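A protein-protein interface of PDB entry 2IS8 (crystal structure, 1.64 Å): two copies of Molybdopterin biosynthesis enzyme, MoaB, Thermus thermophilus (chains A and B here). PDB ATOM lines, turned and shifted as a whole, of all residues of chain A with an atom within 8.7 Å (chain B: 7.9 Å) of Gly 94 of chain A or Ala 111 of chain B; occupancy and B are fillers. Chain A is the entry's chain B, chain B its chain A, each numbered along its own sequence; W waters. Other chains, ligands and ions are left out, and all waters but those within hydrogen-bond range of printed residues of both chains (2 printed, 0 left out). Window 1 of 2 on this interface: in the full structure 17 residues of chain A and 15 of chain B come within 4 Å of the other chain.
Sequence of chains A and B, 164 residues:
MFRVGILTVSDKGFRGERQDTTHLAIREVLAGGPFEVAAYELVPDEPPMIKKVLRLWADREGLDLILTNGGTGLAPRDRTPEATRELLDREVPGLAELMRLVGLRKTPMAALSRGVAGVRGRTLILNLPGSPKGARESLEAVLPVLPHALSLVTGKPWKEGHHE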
ATOM      1  N   GLU A  91      10.903  21.358   9.197  1.00  0.00           N
ATOM      2  CA  GLU A  91      11.308  19.962   9.095  1.00  0.00           C
ATOM      3  C   GLU A  91      11.599  19.312  10.441  1.00  0.00           C
ATOM      4  O   GLU A  91      11.824  19.990  11.444  1.00  0.00           O
ATOM      5  CB  GLU A  91      12.536  19.839   8.191  1.00  0.00           C
ATOM      6  CG  GLU A  91      12.234  20.085   6.727  1.00  0.00           C
ATOM      7  CD  GLU A  91      13.455  19.941   5.847  1.00  0.00           C
ATOM      8  OE1 GLU A  91      14.205  18.955   6.022  1.00  0.00           O
ATOM      9  OE2 GLU A  91      13.654  20.810   4.971  1.00  0.00           O
ATOM     10  N   VAL A  92      11.585  17.982  10.445  1.00  0.00           N
ATOM     11  CA  VAL A  92      11.874  17.205  11.650  1.00  0.00           C
ATOM     12  C   VAL A  92      12.983  16.243  11.226  1.00  0.00           C
ATOM     13  O   VAL A  92      12.750  15.055  10.994  1.00  0.00           O
ATOM     14  CB  VAL A  92      10.631  16.412  12.125  1.00  0.00           C
ATOM     15  CG1 VAL A  92      10.931  15.709  13.446  1.00  0.00           C
ATOM     16  CG2 VAL A  92       9.440  17.350  12.293  1.00  0.00           C
ATOM     17  N   PRO A  93      14.221  16.757  11.120  1.00  0.00           N
ATOM     18  CA  PRO A  93      15.365  15.944  10.708  1.00  0.00           C
ATOM     19  C   PRO A  93      15.534  14.638  11.463  1.00  0.00           C
ATOM     20  O   PRO A  93      15.985  13.653  10.887  1.00  0.00           O
ATOM     21  CB  PRO A  93      16.553  16.891  10.892  1.00  0.00           C
ATOM     22  CG  PRO A  93      16.099  17.810  11.973  1.00  0.00           C
ATOM     23  CD  PRO A  93      14.665  18.079  11.597  1.00  0.00           C
ATOM     24  N   GLY A  94      15.175  14.634  12.747  1.00  0.00           N
ATOM     25  CA  GLY A  94      15.304  13.426  13.547  1.00  0.00           C
ATOM     26  C   GLY A  94      14.546  12.248  12.966  1.00  0.00           C
ATOM     27  O   GLY A  94      14.991  11.101  13.072  1.00  0.00           O
ATOM     28  N   LEU A  95      13.398  12.517  12.356  1.00  0.00           N
ATOM     29  CA  LEU A  95      12.610  11.437  11.767  1.00  0.00           C
ATOM     30  C   LEU A  95      13.231  10.970  10.452  1.00  0.00           C
ATOM     31  O   LEU A  95      13.160   9.789  10.108  1.00  0.00           O
ATOM     32  CB  LEU A  95      11.157  11.891  11.562  1.00  0.00           C
ATOM     33  CG  LEU A  95      10.361  12.088  12.860  1.00  0.00           C
ATOM     34  CD1 LEU A  95       8.960  12.616  12.553  1.00  0.00           C
ATOM     35  CD2 LEU A  95      10.275  10.755  13.608  1.00  0.00           C
ATOM     36  N   ALA A  96      13.842  11.894   9.717  1.00  0.00           N
ATOM     37  CA  ALA A  96      14.502  11.549   8.463  1.00  0.00           C
ATOM     38  C   ALA A  96      15.689  10.637   8.785  1.00  0.00           C
ATOM     39  O   ALA A  96      15.988   9.697   8.052  1.00  0.00           O
ATOM     40  CB  ALA A  96      14.974  12.819   7.750  1.00  0.00           C
ATOM     41  N   GLU A  97      16.359  10.918   9.898  1.00  0.00           N
ATOM     42  CA  GLU A  97      17.501  10.113  10.319  1.00  0.00           C
ATOM     43  C   GLU A  97      17.012   8.721  10.713  1.00  0.00           C
ATOM     44  O   GLU A  97      17.629   7.717  10.370  1.00  0.00           O
ATOM     45  CB  GLU A  97      18.204  10.794  11.499  1.00  0.00           C
ATOM     46  CG  GLU A  97      18.720  12.175  11.151  1.00  0.00           C
ATOM     47  CD  GLU A  97      19.101  13.007  12.361  1.00  0.00           C
ATOM     48  OE1 GLU A  97      18.684  12.663  13.492  1.00  0.00           O
ATOM     49  OE2 GLU A  97      19.804  14.026  12.169  1.00  0.00           O
ATOM     50  N   LEU A  98      15.897   8.655  11.430  1.00  0.00           N
ATOM     51  CA  LEU A  98      15.368   7.353  11.829  1.00  0.00           C
ATOM     52  C   LEU A  98      15.026   6.506  10.608  1.00  0.00           C
ATOM     53  O   LEU A  98      15.288   5.303  10.591  1.00  0.00           O
ATOM     54  CB  LEU A  98      14.121   7.509  12.708  1.00  0.00           C
ATOM     55  CG  LEU A  98      14.310   8.054  14.126  1.00  0.00           C
ATOM     56  CD1 LEU A  98      12.966   8.047  14.836  1.00  0.00           C
ATOM     57  CD2 LEU A  98      15.328   7.210  14.891  1.00  0.00           C
ATOM     58  N   MET A  99      14.444   7.127   9.582  1.00  0.00           N
ATOM     59  CA  MET A  99      14.074   6.385   8.382  1.00  0.00           C
ATOM     60  C   MET A  99      15.281   5.850   7.618  1.00  0.00           C
ATOM     61  O   MET A  99      15.157   4.927   6.815  1.00  0.00           O
ATOM     62  CB  MET A  99      13.192   7.245   7.461  1.00  0.00           C
ATOM     63  CG  MET A  99      11.801   7.514   8.042  1.00  0.00           C
ATOM     64  SD  MET A  99      10.638   8.334   6.927  1.00  0.00           S
ATOM     65  CE  MET A  99      11.346  10.005   6.883  1.00  0.00           C
ATOM     66  N   ARG A 100      16.449   6.434   7.867  1.00  0.00           N
ATOM     67  CA  ARG A 100      17.673   5.975   7.221  1.00  0.00           C
ATOM     68  C   ARG A 100      18.350   4.914   8.090  1.00  0.00           C
ATOM     69  O   ARG A 100      19.434   4.429   7.760  1.00  0.00           O
ATOM     70  CB  ARG A 100      18.633   7.145   6.980  1.00  0.00           C
ATOM     71  CG  ARG A 100      18.310   7.964   5.744  1.00  0.00           C
ATOM     72  CD  ARG A 100      19.428   8.950   5.426  1.00  0.00           C
ATOM     73  NE  ARG A 100      19.404  10.137   6.276  1.00  0.00           N
ATOM     74  CZ  ARG A 100      18.622  11.191   6.062  1.00  0.00           C
ATOM     75  NH1 ARG A 100      17.792  11.206   5.021  1.00  0.00           N
ATOM     76  NH2 ARG A 100      18.679  12.236   6.876  1.00  0.00           N
ATOM     77  N   LEU A 101      17.704   4.568   9.203  1.00  0.00           N
ATOM     78  CA  LEU A 101      18.203   3.545  10.130  1.00  0.00           C
ATOM     79  C   LEU A 101      19.628   3.824  10.606  1.00  0.00           C
ATOM     80  O   LEU A 101      20.422   2.900  10.808  1.00  0.00           O
ATOM     81  CB  LEU A 101      18.163   2.168   9.456  1.00  0.00           C
ATOM     82  CG  LEU A 101      16.894   1.796   8.683  1.00  0.00           C
ATOM     83  CD1 LEU A 101      17.067   0.414   8.059  1.00  0.00           C
ATOM     84  CD2 LEU A 101      15.689   1.831   9.605  1.00  0.00           C
ATOM     85  N   VAL A 102      19.939   5.101  10.801  1.00  0.00           N
ATOM     86  CA  VAL A 102      21.273   5.528  11.221  1.00  0.00           C
ATOM     87  C   VAL A 102      21.754   4.930  12.538  1.00  0.00           C
ATOM     88  O   VAL A 102      21.082   5.034  13.563  1.00  0.00           O
ATOM     89  CB  VAL A 102      21.344   7.064  11.348  1.00  0.00           C
ATOM     90  CG1 VAL A 102      22.770   7.495  11.665  1.00  0.00           C
ATOM     91  CG2 VAL A 102      20.858   7.717  10.074  1.00  0.00           C
ATOM     92  N   VAL A 116      12.625  13.267   3.351  1.00  0.00           N
ATOM     93  CA  VAL A 116      12.579  14.242   4.436  1.00  0.00           C
ATOM     94  C   VAL A 116      11.355  13.995   5.307  1.00  0.00           C
ATOM     95  O   VAL A 116      10.508  13.153   4.995  1.00  0.00           O
ATOM     96  CB  VAL A 116      12.504  15.705   3.908  1.00  0.00           C
ATOM     97  CG1 VAL A 116      13.692  15.996   2.995  1.00  0.00           C
ATOM     98  CG2 VAL A 116      11.188  15.941   3.174  1.00  0.00           C
ATOM     99  N   ALA A 117      11.278  14.733   6.408  1.00  0.00           N
ATOM    100  CA  ALA A 117      10.152  14.650   7.323  1.00  0.00           C
ATOM    101  C   ALA A 117       9.880  16.073   7.774  1.00  0.00           C
ATOM    102  O   ALA A 117      10.814  16.841   8.020  1.00  0.00           O
ATOM    103  CB  ALA A 117      10.496  13.771   8.524  1.00  0.00           C
ATOM    104  N   GLY A 118       8.612  16.435   7.874  1.00  0.00           N
ATOM    105  CA  GLY A 118       8.294  17.780   8.298  1.00  0.00           C
ATOM    106  C   GLY A 118       6.824  17.987   8.572  1.00  0.00           C
ATOM    107  O   GLY A 118       6.012  17.065   8.468  1.00  0.00           O
ATOM    108  N   LEU A 126       6.033  12.286   6.146  1.00  0.00           N
ATOM    109  CA  LEU A 126       7.282  11.528   6.087  1.00  0.00           C
ATOM    110  C   LEU A 126       7.446  10.864   4.721  1.00  0.00           C
ATOM    111  O   LEU A 126       6.496  10.276   4.202  1.00  0.00           O
ATOM    112  CB  LEU A 126       7.308  10.426   7.158  1.00  0.00           C
ATOM    113  CG  LEU A 126       7.714  10.773   8.596  1.00  0.00           C
ATOM    114  CD1 LEU A 126       6.739  11.751   9.204  1.00  0.00           C
ATOM    115  CD2 LEU A 126       7.778   9.485   9.413  1.00  0.00           C
ATOM    116  N   ALA A 141      11.114   2.007  12.224  1.00  0.00           N
ATOM    117  CA  ALA A 141      12.104   2.779  12.966  1.00  0.00           C
ATOM    118  C   ALA A 141      11.473   3.995  13.642  1.00  0.00           C
ATOM    119  O   ALA A 141      11.870   4.376  14.741  1.00  0.00           O
ATOM    120  CB  ALA A 141      13.232   3.223  12.038  1.00  0.00           C
ATOM    121  N   VAL A 142      10.489   4.611  12.989  1.00  0.00           N
ATOM    122  CA  VAL A 142       9.841   5.779  13.576  1.00  0.00           C
ATOM    123  C   VAL A 142       8.609   5.439  14.417  1.00  0.00           C
ATOM    124  O   VAL A 142       8.199   6.224  15.267  1.00  0.00           O
ATOM    125  CB  VAL A 142       9.416   6.813  12.484  1.00  0.00           C
ATOM    126  CG1 VAL A 142      10.632   7.244  11.669  1.00  0.00           C
ATOM    127  CG2 VAL A 142       8.352   6.227  11.590  1.00  0.00           C
ATOM    128  N   VAL A 145       7.926   6.430  18.270  1.00  0.00           N
ATOM    129  CA  VAL A 145       7.737   7.823  18.649  1.00  0.00           C
ATOM    130  C   VAL A 145       6.714   8.520  17.761  1.00  0.00           C
ATOM    131  O   VAL A 145       6.474   9.712  17.913  1.00  0.00           O
ATOM    132  CB  VAL A 145       9.065   8.616  18.571  1.00  0.00           C
ATOM    133  CG1 VAL A 145      10.111   7.965  19.464  1.00  0.00           C
ATOM    134  CG2 VAL A 145       9.565   8.686  17.128  1.00  0.00           C
ATOM    135  N   HIS A 148       3.446   9.942  19.735  1.00  0.00           N
ATOM    136  CA  HIS A 148       3.810  11.124  20.512  1.00  0.00           C
ATOM    137  C   HIS A 148       4.014  12.319  19.584  1.00  0.00           C
ATOM    138  O   HIS A 148       3.559  13.431  19.866  1.00  0.00           O
ATOM    139  CB  HIS A 148       5.091  10.868  21.311  1.00  0.00           C
ATOM    140  CG  HIS A 148       5.452  11.985  22.242  1.00  0.00           C
ATOM    141  ND1 HIS A 148       4.866  12.141  23.484  1.00  0.00           N
ATOM    142  CD2 HIS A 148       6.316  13.019  22.108  1.00  0.00           C
ATOM    143  CE1 HIS A 148       5.355  13.217  24.069  1.00  0.00           C
ATOM    144  NE2 HIS A 148       6.237  13.771  23.256  1.00  0.00           N
ATOM    145  N   ALA A 149       4.702  12.076  18.473  1.00  0.00           N
ATOM    146  CA  ALA A 149       4.962  13.118  17.488  1.00  0.00           C
ATOM    147  C   ALA A 149       3.652  13.690  16.958  1.00  0.00           C
ATOM    148  O   ALA A 149       3.480  14.910  16.877  1.00  0.00           O
ATOM    149  CB  ALA A 149       5.776  12.549  16.332  1.00  0.00           C
ATOM    150  N   THR B  72      12.042  23.029  21.310  1.00  0.00           N
ATOM    151  CA  THR B  72      12.599  22.385  20.122  1.00  0.00           C
ATOM    152  C   THR B  72      11.713  21.266  19.586  1.00  0.00           C
ATOM    153  O   THR B  72      12.050  20.632  18.582  1.00  0.00           O
ATOM    154  CB  THR B  72      13.985  21.773  20.394  1.00  0.00           C
ATOM    155  OG1 THR B  72      13.854  20.715  21.350  1.00  0.00           O
ATOM    156  CG2 THR B  72      14.948  22.828  20.928  1.00  0.00           C
ATOM    157  N   LEU B  74       7.812  19.379  18.461  1.00  0.00           N
ATOM    158  CA  LEU B  74       6.914  19.460  17.317  1.00  0.00           C
ATOM    159  C   LEU B  74       5.632  20.247  17.554  1.00  0.00           C
ATOM    160  O   LEU B  74       4.796  20.351  16.653  1.00  0.00           O
ATOM    161  CB  LEU B  74       6.574  18.044  16.832  1.00  0.00           C
ATOM    162  CG  LEU B  74       7.601  17.401  15.891  1.00  0.00           C
ATOM    163  CD1 LEU B  74       8.987  17.470  16.481  1.00  0.00           C
ATOM    164  CD2 LEU B  74       7.212  15.960  15.618  1.00  0.00           C
ATOM    165  N   ALA B  96      23.831  18.527  16.521  1.00  0.00           N
ATOM    166  CA  ALA B  96      22.382  18.425  16.562  1.00  0.00           C
ATOM    167  C   ALA B  96      22.020  16.939  16.546  1.00  0.00           C
ATOM    168  O   ALA B  96      21.069  16.520  17.193  1.00  0.00           O
ATOM    169  CB  ALA B  96      21.770  19.146  15.358  1.00  0.00           C
ATOM    170  N   GLU B  97      22.790  16.151  15.801  1.00  0.00           N
ATOM    171  CA  GLU B  97      22.560  14.713  15.716  1.00  0.00           C
ATOM    172  C   GLU B  97      22.861  14.067  17.068  1.00  0.00           C
ATOM    173  O   GLU B  97      22.092  13.241  17.559  1.00  0.00           O
ATOM    174  CB  GLU B  97      23.448  14.112  14.623  1.00  0.00           C
ATOM    175  CG  GLU B  97      23.048  14.552  13.216  1.00  0.00           C
ATOM    176  CD  GLU B  97      24.140  14.339  12.178  1.00  0.00           C
ATOM    177  OE1 GLU B  97      25.264  13.946  12.557  1.00  0.00           O
ATOM    178  OE2 GLU B  97      23.872  14.582  10.982  1.00  0.00           O
ATOM    179  N   MET B  99      22.647  15.333  19.978  1.00  0.00           N
ATOM    180  CA  MET B  99      21.589  15.695  20.920  1.00  0.00           C
ATOM    181  C   MET B  99      20.300  14.902  20.702  1.00  0.00           C
ATOM    182  O   MET B  99      19.450  14.837  21.591  1.00  0.00           O
ATOM    183  CB  MET B  99      21.293  17.198  20.853  1.00  0.00           C
ATOM    184  CG  MET B  99      22.471  18.074  21.268  1.00  0.00           C
ATOM    185  SD  MET B  99      22.008  19.822  21.519  1.00  0.00           S
ATOM    186  CE  MET B  99      21.870  20.411  19.799  1.00  0.00           C
ATOM    187  N   ARG B 100      20.147  14.319  19.518  1.00  0.00           N
ATOM    188  CA  ARG B 100      18.978  13.497  19.232  1.00  0.00           C
ATOM    189  C   ARG B 100      19.252  12.044  19.619  1.00  0.00           C
ATOM    190  O   ARG B 100      18.413  11.166  19.404  1.00  0.00           O
ATOM    191  CB  ARG B 100      18.589  13.590  17.756  1.00  0.00           C
ATOM    192  CG  ARG B 100      17.815  14.851  17.429  1.00  0.00           C
ATOM    193  CD  ARG B 100      17.218  14.775  16.040  1.00  0.00           C
ATOM    194  NE  ARG B 100      18.195  15.017  14.984  1.00  0.00           N
ATOM    195  CZ  ARG B 100      18.572  16.229  14.594  1.00  0.00           C
ATOM    196  NH1 ARG B 100      18.053  17.298  15.184  1.00  0.00           N
ATOM    197  NH2 ARG B 100      19.434  16.375  13.596  1.00  0.00           N
ATOM    198  N   LEU B 101      20.431  11.804  20.188  1.00  0.00           N
ATOM    199  CA  LEU B 101      20.835  10.472  20.646  1.00  0.00           C
ATOM    200  C   LEU B 101      20.659   9.422  19.549  1.00  0.00           C
ATOM    201  O   LEU B 101      20.236   8.293  19.815  1.00  0.00           O
ATOM    202  CB  LEU B 101      20.010  10.070  21.879  1.00  0.00           C
ATOM    203  CG  LEU B 101      19.823  11.124  22.982  1.00  0.00           C
ATOM    204  CD1 LEU B 101      19.068  10.497  24.157  1.00  0.00           C
ATOM    205  CD2 LEU B 101      21.164  11.659  23.444  1.00  0.00           C
ATOM    206  N   VAL B 102      20.991   9.796  18.318  1.00  0.00           N
ATOM    207  CA  VAL B 102      20.847   8.899  17.173  1.00  0.00           C
ATOM    208  C   VAL B 102      21.673   7.629  17.318  1.00  0.00           C
ATOM    209  O   VAL B 102      22.851   7.677  17.674  1.00  0.00           O
ATOM    210  CB  VAL B 102      21.262   9.596  15.862  1.00  0.00           C
ATOM    211  CG1 VAL B 102      20.979   8.685  14.674  1.00  0.00           C
ATOM    212  CG2 VAL B 102      20.519  10.912  15.708  1.00  0.00           C
ATOM    213  N   THR B 107      14.296   3.383  19.696  1.00  0.00           N
ATOM    214  CA  THR B 107      14.028   4.724  19.179  1.00  0.00           C
ATOM    215  C   THR B 107      13.809   5.718  20.315  1.00  0.00           C
ATOM    216  O   THR B 107      12.878   5.582  21.111  1.00  0.00           O
ATOM    217  CB  THR B 107      12.797   4.731  18.268  1.00  0.00           C
ATOM    218  OG1 THR B 107      12.994   3.800  17.195  1.00  0.00           O
ATOM    219  CG2 THR B 107      12.579   6.117  17.692  1.00  0.00           C
ATOM    220  N   PRO B 108      14.669   6.743  20.399  1.00  0.00           N
ATOM    221  CA  PRO B 108      14.561   7.752  21.454  1.00  0.00           C
ATOM    222  C   PRO B 108      13.586   8.879  21.144  1.00  0.00           C
ATOM    223  O   PRO B 108      13.416   9.270  19.984  1.00  0.00           O
ATOM    224  CB  PRO B 108      15.993   8.258  21.577  1.00  0.00           C
ATOM    225  CG  PRO B 108      16.428   8.276  20.140  1.00  0.00           C
ATOM    226  CD  PRO B 108      15.907   6.937  19.617  1.00  0.00           C
ATOM    227  N   MET B 109      12.945   9.394  22.189  1.00  0.00           N
ATOM    228  CA  MET B 109      12.021  10.505  22.030  1.00  0.00           C
ATOM    229  C   MET B 109      12.843  11.722  21.638  1.00  0.00           C
ATOM    230  O   MET B 109      12.313  12.697  21.106  1.00  0.00           O
ATOM    231  CB  MET B 109      11.288  10.785  23.343  1.00  0.00           C
ATOM    232  CG  MET B 109      10.188   9.793  23.676  1.00  0.00           C
ATOM    233  SD  MET B 109       8.760   9.997  22.588  1.00  0.00           S
ATOM    234  CE  MET B 109       7.932   8.419  22.794  1.00  0.00           C
ATOM    235  N   ALA B 110      14.147  11.658  21.900  1.00  0.00           N
ATOM    236  CA  ALA B 110      15.044  12.765  21.560  1.00  0.00           C
ATOM    237  C   ALA B 110      15.062  13.002  20.053  1.00  0.00           C
ATOM    238  O   ALA B 110      15.426  14.084  19.590  1.00  0.00           O
ATOM    239  CB  ALA B 110      16.460  12.482  22.061  1.00  0.00           C
ATOM    240  N   ALA B 111      14.674  11.989  19.284  1.00  0.00           N
ATOM    241  CA  ALA B 111      14.636  12.129  17.835  1.00  0.00           C
ATOM    242  C   ALA B 111      13.604  13.193  17.451  1.00  0.00           C
ATOM    243  O   ALA B 111      13.622  13.713  16.329  1.00  0.00           O
ATOM    244  CB  ALA B 111      14.285  10.787  17.181  1.00  0.00           C
ATOM    245  N   LEU B 112      12.706  13.518  18.377  1.00  0.00           N
ATOM    246  CA  LEU B 112      11.683  14.520  18.102  1.00  0.00           C
ATOM    247  C   LEU B 112      12.134  15.934  18.438  1.00  0.00           C
ATOM    248  O   LEU B 112      11.322  16.858  18.465  1.00  0.00           O
ATOM    249  CB  LEU B 112      10.397  14.200  18.858  1.00  0.00           C
ATOM    250  CG  LEU B 112       9.767  12.846  18.523  1.00  0.00           C
ATOM    251  CD1 LEU B 112       8.459  12.715  19.285  1.00  0.00           C
ATOM    252  CD2 LEU B 112       9.528  12.731  17.018  1.00  0.00           C
ATOM    253  N   SER B 113      13.422  16.115  18.709  1.00  0.00           N
ATOM    254  CA  SER B 113      13.925  17.460  18.981  1.00  0.00           C
ATOM    255  C   SER B 113      14.466  18.044  17.682  1.00  0.00           C
ATOM    256  O   SER B 113      15.273  17.411  16.997  1.00  0.00           O
ATOM    257  CB  SER B 113      15.043  17.441  20.019  1.00  0.00           C
ATOM    258  OG  SER B 113      15.565  18.755  20.183  1.00  0.00           O
ATOM    259  N   ARG B 114      14.025  19.256  17.351  1.00  0.00           N
ATOM    260  CA  ARG B 114      14.465  19.920  16.133  1.00  0.00           C
ATOM    261  C   ARG B 114      15.593  20.903  16.432  1.00  0.00           C
ATOM    262  O   ARG B 114      15.970  21.703  15.580  1.00  0.00           O
ATOM    263  CB  ARG B 114      13.291  20.663  15.491  1.00  0.00           C
ATOM    264  CG  ARG B 114      12.106  19.771  15.167  1.00  0.00           C
ATOM    265  CD  ARG B 114      10.971  20.567  14.545  1.00  0.00           C
ATOM    266  NE  ARG B 114      10.557  21.687  15.388  1.00  0.00           N
ATOM    267  CZ  ARG B 114      10.879  22.956  15.151  1.00  0.00           C
ATOM    268  NH1 ARG B 114      11.620  23.272  14.099  1.00  0.00           N
ATOM    269  NH2 ARG B 114      10.449  23.913  15.959  1.00  0.00           N
ATOM    270  N   GLY B 115      16.129  20.832  17.645  1.00  0.00           N
ATOM    271  CA  GLY B 115      17.205  21.733  18.023  1.00  0.00           C
ATOM    272  C   GLY B 115      18.390  21.729  17.075  1.00  0.00           C
ATOM    273  O   GLY B 115      18.796  20.684  16.554  1.00  0.00           O
ATOM    274  N   PRO B 129      16.868  19.870  24.377  1.00  0.00           N
ATOM    275  CA  PRO B 129      15.436  19.650  24.591  1.00  0.00           C
ATOM    276  C   PRO B 129      15.081  20.289  25.943  1.00  0.00           C
ATOM    277  O   PRO B 129      15.970  20.515  26.763  1.00  0.00           O
ATOM    278  CB  PRO B 129      15.320  18.124  24.619  1.00  0.00           C
ATOM    279  CG  PRO B 129      16.429  17.686  23.707  1.00  0.00           C
ATOM    280  CD  PRO B 129      17.568  18.601  24.108  1.00  0.00           C
ATOM    281  N   SER B 138      20.857  14.892  26.279  1.00  0.00           N
ATOM    282  CA  SER B 138      21.416  15.469  25.060  1.00  0.00           C
ATOM    283  C   SER B 138      22.760  16.155  25.339  1.00  0.00           C
ATOM    284  O   SER B 138      23.682  16.073  24.529  1.00  0.00           O
ATOM    285  CB  SER B 138      20.433  16.472  24.451  1.00  0.00           C
ATOM    286  OG  SER B 138      19.250  15.816  24.019  1.00  0.00           O
HETATM  287  O   HOH W   1      13.164  22.143  12.075  1.00  0.00           O
HETATM  288  O   HOH W   2      13.984  16.211  14.764  1.00  0.00           O
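Of chain B, only Arg 100 and Ala 111 come within 4 Å of Gly 94 of chain A. Of chain A, only Gly 94 and Leu 98 come within 4 Å of Ala 111 of chain B. Of the printed residues of chain B, Pro 93 of chain A touches Arg 100. Of the printed residues of chain A, Leu 112 of chain B touches Val 145, His 148 and Ala 149. Of the printed residues of chain A, Met 109 of chain B touches Val 145 and His 148. Of the printed residues of chain B, Glu 91 of chain A touches Arg 114 (3.3 Å). Of the printed residues of chain A, Val 102 of chain B touches Glu 97 (3.4 Å) and Val 102 (3.7 Å). Leu 126 of chain A touches none of the printed residues of chain B. Ser 113 of chain B touches none of the printed residues of chain A. The nearest residue of chain B that does not touch Gly 94 of chain A is Ser 113 of chain B (5.1 Å).
The guanidinium group of Arg 100 of chain B lies within salt-bridge range of the side-chain carboxylate of Glu 97 of chain A, at 2.8 Å. The side-chain hydroxyl (OG1) of Thr 107 of chain B lies within hydrogen-bond range of the backbone carbonyl oxygen (O) of Ala 141 of chain A, at 2.8 Å.
Among the printed residues, merely in contact across the chains: Glu 91 of chain A with Arg 114 of chain B, Pro 93 of chain A with Arg 100 of chain B, Gly 94 of chain A with Arg 100 of chain B, Gly 94 of chain A with Ala 111 of chain B, Glu 97 of chain A with Glu 97 of chain B, Glu 97 of chain A with Val 102 of chain B, Leu 98 of chain A with Thr 107 of chain B, Leu 98 of chain A with Ala 111 of chain B, Val 102 of chain A with Val 102 of chain B, Val 145 of chain A with Thr 107 of chain B, Val 145 of chain A with Pro 108 of chain B, Val 145 of chain A with Met 109 of chain B, Val 145 of chain A with Leu 112 of chain B, His 148 of chain A with Met 109 of chain B, His 148 of chain A with Leu 112 of chain B, Ala 149 of chain A with Leu 74 of chain B and Ala 149 of chain A with Leu 112 of chain B.
Of the 19 printed residues of chain B, 10 touch a printed residue of chain A. Hydrophobic or aromatic side chains of chain B within 4 Å of the printed part of chain A: Leu 74, Val 102, Met 109, Ala 111 and Leu 112. Of the 21 printed residues of chain A, 10 touch a printed residue of chain B. Printed residues of chain A that touch a printed residue of chain B: Glu 91, Pro 93, Gly 94, Glu 97, Leu 98, Val 102, Ala 141, Val 145, His 148 and Ala 149. Among the printed residues, 19 pairs touch across the chains. Among the printed residues, Asp or Glu carboxylates within 4 Å of a Lys or Arg side-chain nitrogen of the other chain: Glu 97 of chain A with Arg 100 of chain B (2.8 Å).
O of Thr 72 of chain B sits at hydrogen-bond distance from N of Arg 114 of chain B (2.7 Å). The guanidinium group (NH1) of Arg 100 of chain B lies within hydrogen-bond range of the backbone carbonyl oxygen (O) of Ser 113 of chain B (3.3 Å).
Water W1 lies within hydrogen-bond range of the backbone carbonyl oxygen of Glu 91 of chain A (2.6 Å) and the guanidinium group of Arg 114 of chain B (2.8 Å). Water W2 lies within hydrogen-bond range of N of Gly 94 of chain A (2.8 Å), O of Ser 113 of chain B (2.8 Å) and O of Ala 111 of chain B (3.0 Å).
Glu 97 of chain B touches its own counterpart, Glu 97 of chain A. Glu 97 of chain A touches Arg 100 of chain B, but with the chains exchanged Arg 100 of chain A does not touch Glu 97 of chain B (7.0 Å). Glu 97 of chain A touches Val 102 of chain B, but with the chains exchanged Val 102 of chain A does not touch Glu 97 of chain B (7.0 Å). Val 102 of chain B touches its own counterpart, Val 102 of chain A. Positions printed for both chains: 96, 97, 99, 100, 101 and 102. Of the 19 pairs that touch across the chains among the printed residues, 2 have their exchanged pair printed and touching as well.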
